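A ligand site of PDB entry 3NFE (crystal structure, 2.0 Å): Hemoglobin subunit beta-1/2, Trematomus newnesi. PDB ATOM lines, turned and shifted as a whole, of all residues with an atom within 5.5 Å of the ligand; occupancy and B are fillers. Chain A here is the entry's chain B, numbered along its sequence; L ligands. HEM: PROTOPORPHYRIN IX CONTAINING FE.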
ATOM      1  N   THR A  38       9.224 -37.915   8.043  1.00  0.00           N
ATOM      2  CA  THR A  38       8.519 -36.704   8.468  1.00  0.00           C
ATOM      3  C   THR A  38       7.345 -36.460   7.537  1.00  0.00           C
ATOM      4  O   THR A  38       6.397 -35.737   7.859  1.00  0.00           O
ATOM      5  CB  THR A  38       9.436 -35.477   8.536  1.00  0.00           C
ATOM      6  OG1 THR A  38      10.195 -35.347   7.329  1.00  0.00           O
ATOM      7  CG2 THR A  38      10.496 -35.605   9.630  1.00  0.00           C
ATOM      8  N   TYR A  41       3.155 -36.669   8.457  1.00  0.00           N
ATOM      9  CA  TYR A  41       2.229 -35.681   9.008  1.00  0.00           C
ATOM     10  C   TYR A  41       1.713 -34.704   7.970  1.00  0.00           C
ATOM     11  O   TYR A  41       0.979 -33.772   8.324  1.00  0.00           O
ATOM     12  CB  TYR A  41       2.951 -34.930  10.145  1.00  0.00           C
ATOM     13  CG  TYR A  41       3.640 -35.866  11.122  1.00  0.00           C
ATOM     14  CD1 TYR A  41       5.010 -36.086  11.058  1.00  0.00           C
ATOM     15  CD2 TYR A  41       2.928 -36.530  12.108  1.00  0.00           C
ATOM     16  CE1 TYR A  41       5.633 -36.939  11.958  1.00  0.00           C
ATOM     17  CE2 TYR A  41       3.542 -37.383  13.005  1.00  0.00           C
ATOM     18  CZ  TYR A  41       4.900 -37.582  12.915  1.00  0.00           C
ATOM     19  OH  TYR A  41       5.504 -38.436  13.808  1.00  0.00           O
ATOM     20  N   PHE A  42       2.065 -34.863   6.698  1.00  0.00           N
ATOM     21  CA  PHE A  42       1.632 -33.858   5.724  1.00  0.00           C
ATOM     22  C   PHE A  42       0.916 -34.498   4.549  1.00  0.00           C
ATOM     23  O   PHE A  42       1.286 -34.359   3.377  1.00  0.00           O
ATOM     24  CB  PHE A  42       2.842 -33.037   5.262  1.00  0.00           C
ATOM     25  CG  PHE A  42       3.529 -32.306   6.407  1.00  0.00           C
ATOM     26  CD1 PHE A  42       2.913 -31.241   7.045  1.00  0.00           C
ATOM     27  CD2 PHE A  42       4.779 -32.699   6.850  1.00  0.00           C
ATOM     28  CE1 PHE A  42       3.527 -30.588   8.096  1.00  0.00           C
ATOM     29  CE2 PHE A  42       5.406 -32.045   7.895  1.00  0.00           C
ATOM     30  CZ  PHE A  42       4.775 -30.980   8.517  1.00  0.00           C
ATOM     31  N   PHE A  45      -0.849 -32.031   1.598  1.00  0.00           N
ATOM     32  CA  PHE A  45       0.022 -31.143   0.848  1.00  0.00           C
ATOM     33  C   PHE A  45       0.141 -31.486  -0.634  1.00  0.00           C
ATOM     34  O   PHE A  45       0.476 -30.606  -1.437  1.00  0.00           O
ATOM     35  CB  PHE A  45       1.417 -31.140   1.484  1.00  0.00           C
ATOM     36  CG  PHE A  45       1.510 -30.312   2.759  1.00  0.00           C
ATOM     37  CD1 PHE A  45       0.439 -30.253   3.638  1.00  0.00           C
ATOM     38  CD2 PHE A  45       2.650 -29.611   3.070  1.00  0.00           C
ATOM     39  CE1 PHE A  45       0.507 -29.512   4.806  1.00  0.00           C
ATOM     40  CE2 PHE A  45       2.722 -28.850   4.229  1.00  0.00           C
ATOM     41  CZ  PHE A  45       1.652 -28.801   5.108  1.00  0.00           C
ATOM     42  N   HIS A  63       4.320 -23.802   4.724  1.00  0.00           N
ATOM     43  CA  HIS A  63       4.441 -24.327   6.083  1.00  0.00           C
ATOM     44  C   HIS A  63       5.853 -24.221   6.621  1.00  0.00           C
ATOM     45  O   HIS A  63       6.093 -24.102   7.827  1.00  0.00           O
ATOM     46  CB  HIS A  63       3.978 -25.777   6.107  1.00  0.00           C
ATOM     47  CG  HIS A  63       3.709 -26.301   7.479  1.00  0.00           C
ATOM     48  ND1 HIS A  63       2.712 -25.811   8.290  1.00  0.00           N
ATOM     49  CD2 HIS A  63       4.299 -27.290   8.181  1.00  0.00           C
ATOM     50  CE1 HIS A  63       2.699 -26.459   9.435  1.00  0.00           C
ATOM     51  NE2 HIS A  63       3.664 -27.370   9.404  1.00  0.00           N
ATOM     52  N   LYS A  66       5.778 -20.787   8.100  1.00  0.00           N
ATOM     53  CA  LYS A  66       5.148 -20.700   9.425  1.00  0.00           C
ATOM     54  C   LYS A  66       6.089 -21.258  10.485  1.00  0.00           C
ATOM     55  O   LYS A  66       6.333 -20.654  11.523  1.00  0.00           O
ATOM     56  CB  LYS A  66       3.798 -21.419   9.441  1.00  0.00           C
ATOM     57  CG  LYS A  66       2.641 -20.612  10.006  1.00  0.00           C
ATOM     58  CD  LYS A  66       1.325 -21.357   9.874  1.00  0.00           C
ATOM     59  CE  LYS A  66       0.386 -21.085  11.033  1.00  0.00           C
ATOM     60  NZ  LYS A  66      -0.873 -21.873  10.975  1.00  0.00           N
ATOM     61  N   VAL A  67       6.625 -22.452  10.220  1.00  0.00           N
ATOM     62  CA  VAL A  67       7.462 -23.147  11.184  1.00  0.00           C
ATOM     63  C   VAL A  67       8.613 -22.270  11.642  1.00  0.00           C
ATOM     64  O   VAL A  67       8.945 -22.190  12.828  1.00  0.00           O
ATOM     65  CB  VAL A  67       8.033 -24.463  10.598  1.00  0.00           C
ATOM     66  CG1 VAL A  67       9.037 -25.049  11.573  1.00  0.00           C
ATOM     67  CG2 VAL A  67       6.943 -25.465  10.288  1.00  0.00           C
ATOM     68  N   GLY A  70       7.781 -19.645  13.937  1.00  0.00           N
ATOM     69  CA  GLY A  70       7.588 -20.376  15.162  1.00  0.00           C
ATOM     70  C   GLY A  70       8.709 -20.162  16.159  1.00  0.00           C
ATOM     71  O   GLY A  70       8.521 -20.332  17.356  1.00  0.00           O
ATOM     72  N   LEU A  71       9.882 -19.791  15.671  1.00  0.00           N
ATOM     73  CA  LEU A  71      11.025 -19.524  16.529  1.00  0.00           C
ATOM     74  C   LEU A  71      11.005 -18.075  17.017  1.00  0.00           C
ATOM     75  O   LEU A  71      11.696 -17.649  17.942  1.00  0.00           O
ATOM     76  CB  LEU A  71      12.343 -19.736  15.782  1.00  0.00           C
ATOM     77  CG  LEU A  71      12.577 -21.090  15.099  1.00  0.00           C
ATOM     78  CD1 LEU A  71      13.785 -21.028  14.169  1.00  0.00           C
ATOM     79  CD2 LEU A  71      12.737 -22.157  16.171  1.00  0.00           C
ATOM     80  N   ARG A  73       8.761 -16.282  18.585  1.00  0.00           N
ATOM     81  CA  ARG A  73       8.382 -16.056  19.987  1.00  0.00           C
ATOM     82  C   ARG A  73       9.605 -16.280  20.874  1.00  0.00           C
ATOM     83  O   ARG A  73       9.901 -15.533  21.807  1.00  0.00           O
ATOM     84  CB  ARG A  73       7.215 -16.946  20.389  1.00  0.00           C
ATOM     85  CG  ARG A  73       7.153 -18.331  19.808  1.00  0.00           C
ATOM     86  CD  ARG A  73       5.777 -18.975  20.008  1.00  0.00           C
ATOM     87  NE  ARG A  73       5.046 -19.013  18.746  1.00  0.00           N
ATOM     88  CZ  ARG A  73       3.868 -19.556  18.510  1.00  0.00           C
ATOM     89  NH1 ARG A  73       3.194 -20.170  19.481  1.00  0.00           N
ATOM     90  NH2 ARG A  73       3.331 -19.505  17.303  1.00  0.00           N
ATOM     91  N   TYR A  85       6.410 -21.842  24.606  1.00  0.00           N
ATOM     92  CA  TYR A  85       6.004 -22.878  23.646  1.00  0.00           C
ATOM     93  C   TYR A  85       5.002 -23.871  24.204  1.00  0.00           C
ATOM     94  O   TYR A  85       4.621 -24.844  23.544  1.00  0.00           O
ATOM     95  CB  TYR A  85       7.267 -23.607  23.144  1.00  0.00           C
ATOM     96  CG  TYR A  85       7.991 -22.771  22.102  1.00  0.00           C
ATOM     97  CD1 TYR A  85       7.513 -22.688  20.799  1.00  0.00           C
ATOM     98  CD2 TYR A  85       9.147 -22.080  22.429  1.00  0.00           C
ATOM     99  CE1 TYR A  85       8.170 -21.935  19.847  1.00  0.00           C
ATOM    100  CE2 TYR A  85       9.805 -21.327  21.477  1.00  0.00           C
ATOM    101  CZ  TYR A  85       9.319 -21.254  20.193  1.00  0.00           C
ATOM    102  OH  TYR A  85       9.973 -20.491  19.251  1.00  0.00           O
ATOM    103  N   LEU A  88       2.101 -24.320  21.884  1.00  0.00           N
ATOM    104  CA  LEU A  88       2.494 -25.010  20.658  1.00  0.00           C
ATOM    105  C   LEU A  88       2.805 -26.468  20.953  1.00  0.00           C
ATOM    106  O   LEU A  88       2.480 -27.369  20.177  1.00  0.00           O
ATOM    107  CB  LEU A  88       3.691 -24.296  20.059  1.00  0.00           C
ATOM    108  CG  LEU A  88       3.603 -23.909  18.581  1.00  0.00           C
ATOM    109  CD1 LEU A  88       4.977 -23.974  17.945  1.00  0.00           C
ATOM    110  CD2 LEU A  88       2.601 -24.810  17.868  1.00  0.00           C
ATOM    111  N   LEU A  91      -0.362 -28.394  21.299  1.00  0.00           N
ATOM    112  CA  LEU A  91      -0.939 -28.661  19.993  1.00  0.00           C
ATOM    113  C   LEU A  91      -0.208 -29.805  19.301  1.00  0.00           C
ATOM    114  O   LEU A  91      -0.831 -30.731  18.774  1.00  0.00           O
ATOM    115  CB  LEU A  91      -0.894 -27.428  19.089  1.00  0.00           C
ATOM    116  CG  LEU A  91      -1.486 -27.622  17.683  1.00  0.00           C
ATOM    117  CD1 LEU A  91      -3.002 -27.683  17.759  1.00  0.00           C
ATOM    118  CD2 LEU A  91      -1.021 -26.529  16.741  1.00  0.00           C
ATOM    119  N   HIS A  92       1.118 -29.736  19.303  1.00  0.00           N
ATOM    120  CA  HIS A  92       1.903 -30.719  18.560  1.00  0.00           C
ATOM    121  C   HIS A  92       1.667 -32.122  19.088  1.00  0.00           C
ATOM    122  O   HIS A  92       1.686 -33.103  18.333  1.00  0.00           O
ATOM    123  CB  HIS A  92       3.390 -30.331  18.598  1.00  0.00           C
ATOM    124  CG  HIS A  92       3.727 -29.354  17.509  1.00  0.00           C
ATOM    125  ND1 HIS A  92       3.848 -28.008  17.706  1.00  0.00           N
ATOM    126  CD2 HIS A  92       3.957 -29.561  16.190  1.00  0.00           C
ATOM    127  CE1 HIS A  92       4.158 -27.410  16.565  1.00  0.00           C
ATOM    128  NE2 HIS A  92       4.217 -28.337  15.623  1.00  0.00           N
ATOM    129  N   LEU A  96      -1.813 -32.736  16.994  1.00  0.00           N
ATOM    130  CA  LEU A  96      -1.123 -33.167  15.779  1.00  0.00           C
ATOM    131  C   LEU A  96      -0.441 -34.521  15.919  1.00  0.00           C
ATOM    132  O   LEU A  96      -0.250 -35.197  14.916  1.00  0.00           O
ATOM    133  CB  LEU A  96      -0.075 -32.137  15.357  1.00  0.00           C
ATOM    134  CG  LEU A  96      -0.599 -30.729  15.086  1.00  0.00           C
ATOM    135  CD1 LEU A  96       0.578 -29.786  14.914  1.00  0.00           C
ATOM    136  CD2 LEU A  96      -1.489 -30.717  13.850  1.00  0.00           C
ATOM    137  N   VAL A  98       2.683 -35.564  16.703  1.00  0.00           N
ATOM    138  CA  VAL A  98       3.979 -35.669  16.047  1.00  0.00           C
ATOM    139  C   VAL A  98       5.080 -36.154  16.966  1.00  0.00           C
ATOM    140  O   VAL A  98       5.209 -35.712  18.107  1.00  0.00           O
ATOM    141  CB  VAL A  98       4.399 -34.276  15.514  1.00  0.00           C
ATOM    142  CG1 VAL A  98       5.765 -34.391  14.841  1.00  0.00           C
ATOM    143  CG2 VAL A  98       3.353 -33.711  14.564  1.00  0.00           C
ATOM    144  N   ASN A 102      11.435 -35.601  15.817  1.00  0.00           N
ATOM    145  CA  ASN A 102      11.426 -34.919  14.536  1.00  0.00           C
ATOM    146  C   ASN A 102      11.795 -33.443  14.701  1.00  0.00           C
ATOM    147  O   ASN A 102      12.248 -32.839  13.722  1.00  0.00           O
ATOM    148  CB  ASN A 102      10.039 -35.092  13.899  1.00  0.00           C
ATOM    149  CG  ASN A 102       9.867 -36.488  13.328  1.00  0.00           C
ATOM    150  OD1 ASN A 102       8.870 -37.153  13.597  1.00  0.00           O
ATOM    151  ND2 ASN A 102      10.844 -36.929  12.543  1.00  0.00           N
ATOM    152  N   PHE A 103      11.618 -32.872  15.889  1.00  0.00           N
ATOM    153  CA  PHE A 103      11.993 -31.488  16.098  1.00  0.00           C
ATOM    154  C   PHE A 103      13.517 -31.366  15.973  1.00  0.00           C
ATOM    155  O   PHE A 103      14.065 -30.393  15.456  1.00  0.00           O
ATOM    156  CB  PHE A 103      11.555 -30.961  17.464  1.00  0.00           C
ATOM    157  CG  PHE A 103      10.053 -30.995  17.674  1.00  0.00           C
ATOM    158  CD1 PHE A 103       9.211 -30.529  16.692  1.00  0.00           C
ATOM    159  CD2 PHE A 103       9.504 -31.484  18.855  1.00  0.00           C
ATOM    160  CE1 PHE A 103       7.836 -30.543  16.877  1.00  0.00           C
ATOM    161  CE2 PHE A 103       8.135 -31.508  19.052  1.00  0.00           C
ATOM    162  CZ  PHE A 103       7.300 -31.042  18.052  1.00  0.00           C
ATOM    163  N   LEU A 106      14.448 -31.578  12.041  1.00  0.00           N
ATOM    164  CA  LEU A 106      14.142 -30.321  11.389  1.00  0.00           C
ATOM    165  C   LEU A 106      15.037 -29.216  11.938  1.00  0.00           C
ATOM    166  O   LEU A 106      15.460 -28.298  11.212  1.00  0.00           O
ATOM    167  CB  LEU A 106      12.670 -29.964  11.557  1.00  0.00           C
ATOM    168  CG  LEU A 106      12.278 -28.589  10.993  1.00  0.00           C
ATOM    169  CD1 LEU A 106      12.649 -28.522   9.509  1.00  0.00           C
ATOM    170  CD2 LEU A 106      10.804 -28.323  11.221  1.00  0.00           C
ATOM    171  N   SER A 107      15.361 -29.258  13.226  1.00  0.00           N
ATOM    172  CA  SER A 107      16.291 -28.252  13.763  1.00  0.00           C
ATOM    173  C   SER A 107      17.606 -28.305  12.999  1.00  0.00           C
ATOM    174  O   SER A 107      18.097 -27.254  12.580  1.00  0.00           O
ATOM    175  CB  SER A 107      16.550 -28.450  15.247  1.00  0.00           C
ATOM    176  OG  SER A 107      15.424 -28.058  16.028  1.00  0.00           O
ATOM    177  N   ILE A 110      17.305 -26.848   9.572  1.00  0.00           N
ATOM    178  CA  ILE A 110      17.269 -25.368   9.595  1.00  0.00           C
ATOM    179  C   ILE A 110      18.694 -24.852   9.688  1.00  0.00           C
ATOM    180  O   ILE A 110      19.150 -23.935   9.017  1.00  0.00           O
ATOM    181  CB  ILE A 110      16.366 -24.916  10.751  1.00  0.00           C
ATOM    182  CG1 ILE A 110      14.874 -25.137  10.447  1.00  0.00           C
ATOM    183  CG2 ILE A 110      16.595 -23.476  11.173  1.00  0.00           C
ATOM    184  CD1 ILE A 110      14.007 -25.097  11.692  1.00  0.00           C
ATOM    185  N   LEU A 134      18.143 -23.323  19.369  1.00  0.00           N
ATOM    186  CA  LEU A 134      17.202 -24.279  18.807  1.00  0.00           C
ATOM    187  C   LEU A 134      16.984 -25.452  19.744  1.00  0.00           C
ATOM    188  O   LEU A 134      15.875 -25.993  19.834  1.00  0.00           O
ATOM    189  CB  LEU A 134      17.687 -24.745  17.428  1.00  0.00           C
ATOM    190  CG  LEU A 134      17.369 -23.795  16.261  1.00  0.00           C
ATOM    191  CD1 LEU A 134      17.871 -24.373  14.950  1.00  0.00           C
ATOM    192  CD2 LEU A 134      15.869 -23.531  16.191  1.00  0.00           C
ATOM    193  N   VAL A 137      14.428 -24.391  22.202  1.00  0.00           N
ATOM    194  CA  VAL A 137      13.107 -24.454  21.593  1.00  0.00           C
ATOM    195  C   VAL A 137      12.639 -25.890  21.434  1.00  0.00           C
ATOM    196  O   VAL A 137      11.462 -26.242  21.567  1.00  0.00           O
ATOM    197  CB  VAL A 137      13.112 -23.799  20.188  1.00  0.00           C
ATOM    198  CG1 VAL A 137      11.755 -24.001  19.530  1.00  0.00           C
ATOM    199  CG2 VAL A 137      13.470 -22.330  20.243  1.00  0.00           C
ATOM    200  N   VAL A 138      13.584 -26.784  21.117  1.00  0.00           N
ATOM    201  CA  VAL A 138      13.176 -28.168  20.886  1.00  0.00           C
ATOM    202  C   VAL A 138      12.779 -28.830  22.195  1.00  0.00           C
ATOM    203  O   VAL A 138      11.822 -29.602  22.273  1.00  0.00           O
ATOM    204  CB  VAL A 138      14.290 -28.982  20.208  1.00  0.00           C
ATOM    205  CG1 VAL A 138      14.014 -30.477  20.387  1.00  0.00           C
ATOM    206  CG2 VAL A 138      14.414 -28.635  18.733  1.00  0.00           C
ATOM    207  N   LEU A 141       9.261 -27.705  22.932  1.00  0.00           N
ATOM    208  CA  LEU A 141       8.146 -28.326  22.216  1.00  0.00           C
ATOM    209  C   LEU A 141       7.836 -29.738  22.684  1.00  0.00           C
ATOM    210  O   LEU A 141       6.693 -30.195  22.614  1.00  0.00           O
ATOM    211  CB  LEU A 141       8.420 -28.328  20.704  1.00  0.00           C
ATOM    212  CG  LEU A 141       8.492 -26.932  20.071  1.00  0.00           C
ATOM    213  CD1 LEU A 141       9.106 -26.988  18.676  1.00  0.00           C
ATOM    214  CD2 LEU A 141       7.106 -26.299  20.021  1.00  0.00           C
HETATM  215  CHA HEM L   1       1.977 -26.609  13.030  1.00  0.00           C
HETATM  216  CHB HEM L   1       5.998 -24.699  14.891  1.00  0.00           C
HETATM  217  CHC HEM L   1       8.368 -28.810  13.998  1.00  0.00           C
HETATM  218  CHD HEM L   1       4.293 -30.794  12.307  1.00  0.00           C
HETATM  219  C1A HEM L   1       2.880 -25.702  13.523  1.00  0.00           C
HETATM  220  C2A HEM L   1       2.650 -24.286  13.717  1.00  0.00           C
HETATM  221  C3A HEM L   1       3.774 -23.749  14.210  1.00  0.00           C
HETATM  222  C4A HEM L   1       4.738 -24.824  14.346  1.00  0.00           C
HETATM  223  CMA HEM L   1       4.072 -22.289  14.594  1.00  0.00           C
HETATM  224  CAA HEM L   1       1.308 -23.586  13.386  1.00  0.00           C
HETATM  225  CBA HEM L   1       0.172 -23.760  14.374  1.00  0.00           C
HETATM  226  CGA HEM L   1      -0.838 -22.640  14.446  1.00  0.00           C
HETATM  227  O1A HEM L   1      -1.553 -22.444  13.431  1.00  0.00           O
HETATM  228  O2A HEM L   1      -0.909 -21.997  15.526  1.00  0.00           O
HETATM  229  C1B HEM L   1       6.979 -25.669  14.843  1.00  0.00           C
HETATM  230  C2B HEM L   1       8.347 -25.482  15.302  1.00  0.00           C
HETATM  231  C3B HEM L   1       9.022 -26.585  14.985  1.00  0.00           C
HETATM  232  C4B HEM L   1       8.072 -27.530  14.420  1.00  0.00           C
HETATM  233  CMB HEM L   1       8.806 -24.169  15.990  1.00  0.00           C
HETATM  234  CAB HEM L   1      10.477 -26.975  15.313  1.00  0.00           C
HETATM  235  CBB HEM L   1      11.437 -26.058  15.400  1.00  0.00           C
HETATM  236  C1C HEM L   1       7.475 -29.695  13.423  1.00  0.00           C
HETATM  237  C2C HEM L   1       7.818 -30.982  12.848  1.00  0.00           C
HETATM  238  C3C HEM L   1       6.693 -31.539  12.386  1.00  0.00           C
HETATM  239  C4C HEM L   1       5.607 -30.615  12.682  1.00  0.00           C
HETATM  240  CMC HEM L   1       9.267 -31.511  12.763  1.00  0.00           C
HETATM  241  CAC HEM L   1       6.470 -32.903  11.722  1.00  0.00           C
HETATM  242  CBC HEM L   1       7.359 -33.402  10.859  1.00  0.00           C
HETATM  243  C1D HEM L   1       3.323 -29.823  12.295  1.00  0.00           C
HETATM  244  C2D HEM L   1       1.998 -29.937  11.726  1.00  0.00           C
HETATM  245  C3D HEM L   1       1.383 -28.760  11.885  1.00  0.00           C
HETATM  246  C4D HEM L   1       2.279 -27.899  12.621  1.00  0.00           C
HETATM  247  CMD HEM L   1       1.472 -31.220  11.045  1.00  0.00           C
HETATM  248  CAD HEM L   1      -0.064 -28.370  11.539  1.00  0.00           C
HETATM  249  CBD HEM L   1      -0.335 -27.666  10.212  1.00  0.00           C
HETATM  250  CGD HEM L   1      -1.565 -28.146   9.467  1.00  0.00           C
HETATM  251  O1D HEM L   1      -2.675 -27.909  10.004  1.00  0.00           O
HETATM  252  O2D HEM L   1      -1.374 -28.740   8.380  1.00  0.00           O
HETATM  253  NA  HEM L   1       4.167 -26.023  13.928  1.00  0.00           N
HETATM  254  NB  HEM L   1       6.833 -26.926  14.318  1.00  0.00           N
HETATM  255  NC  HEM L   1       6.109 -29.491  13.306  1.00  0.00           N
HETATM  256  ND  HEM L   1       3.468 -28.557  12.852  1.00  0.00           N
HETATM  257 FE   HEM L   1       5.122 -27.789  13.701  1.00  0.00          FE
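A ring nitrogen (NE2) of His 92 binds an iron atom (FE) of the ligand (2.2 Å).
The side-chain amino group (NZ) of Lys 66 lies within salt-bridge range of an oxygen (O1A) of the ligand (2.6 Å).
A ring nitrogen (ND1) of His 92 lies within hydrogen-bond range of the backbone carbonyl oxygen (O) of Leu 88, 2.9 Å away.
N of Val 98 is in hydrogen-bond range of O of His 92, at 3.1 Å.
The backbone carbonyl oxygen of Leu 91 is in hydrogen-bond range of the backbone NH of Leu 96.
O of Phe 103 lies within hydrogen-bond range of OG of Ser 107, 2.8 Å away.
Thr 38 touches the ligand (CB to CBC, 3.7 Å).
CD1 of Tyr 41 touches CAC of the ligand (3.6 Å).
CE1 of Phe 42 touches CMD of the ligand (3.6 Å).
His 63 touches the ligand.
O of Val 67 touches CMB of the ligand (3.7 Å).
NH2 of Arg 73 touches CMA of the ligand, at 3.95 Å.
Leu 88 touches the ligand.
CD2 of Leu 91 touches CBA of the ligand, 3.8 Å away.
Leu 96 touches the ligand (CD1 to C3D, 3.3 Å).
Val 98 touches the ligand.
Asn 102 touches the ligand (O to CMC, 3.4 Å).
Phe 103 touches the ligand.
Leu 106 touches the ligand.
Leu 141 touches the ligand (CD1 to CAB, 3.6 Å).
16 residues have an atom within 4 Å of the ligand: Thr 38, Tyr 41, Phe 42, His 63, Lys 66, Val 67, Arg 73, Leu 88, Leu 91, His 92, Leu 96, Val 98, Asn 102, Phe 103, Leu 106 and Leu 141.
The nearest printed residue that does not touch the ligand is Gly 70 (4.01 Å).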
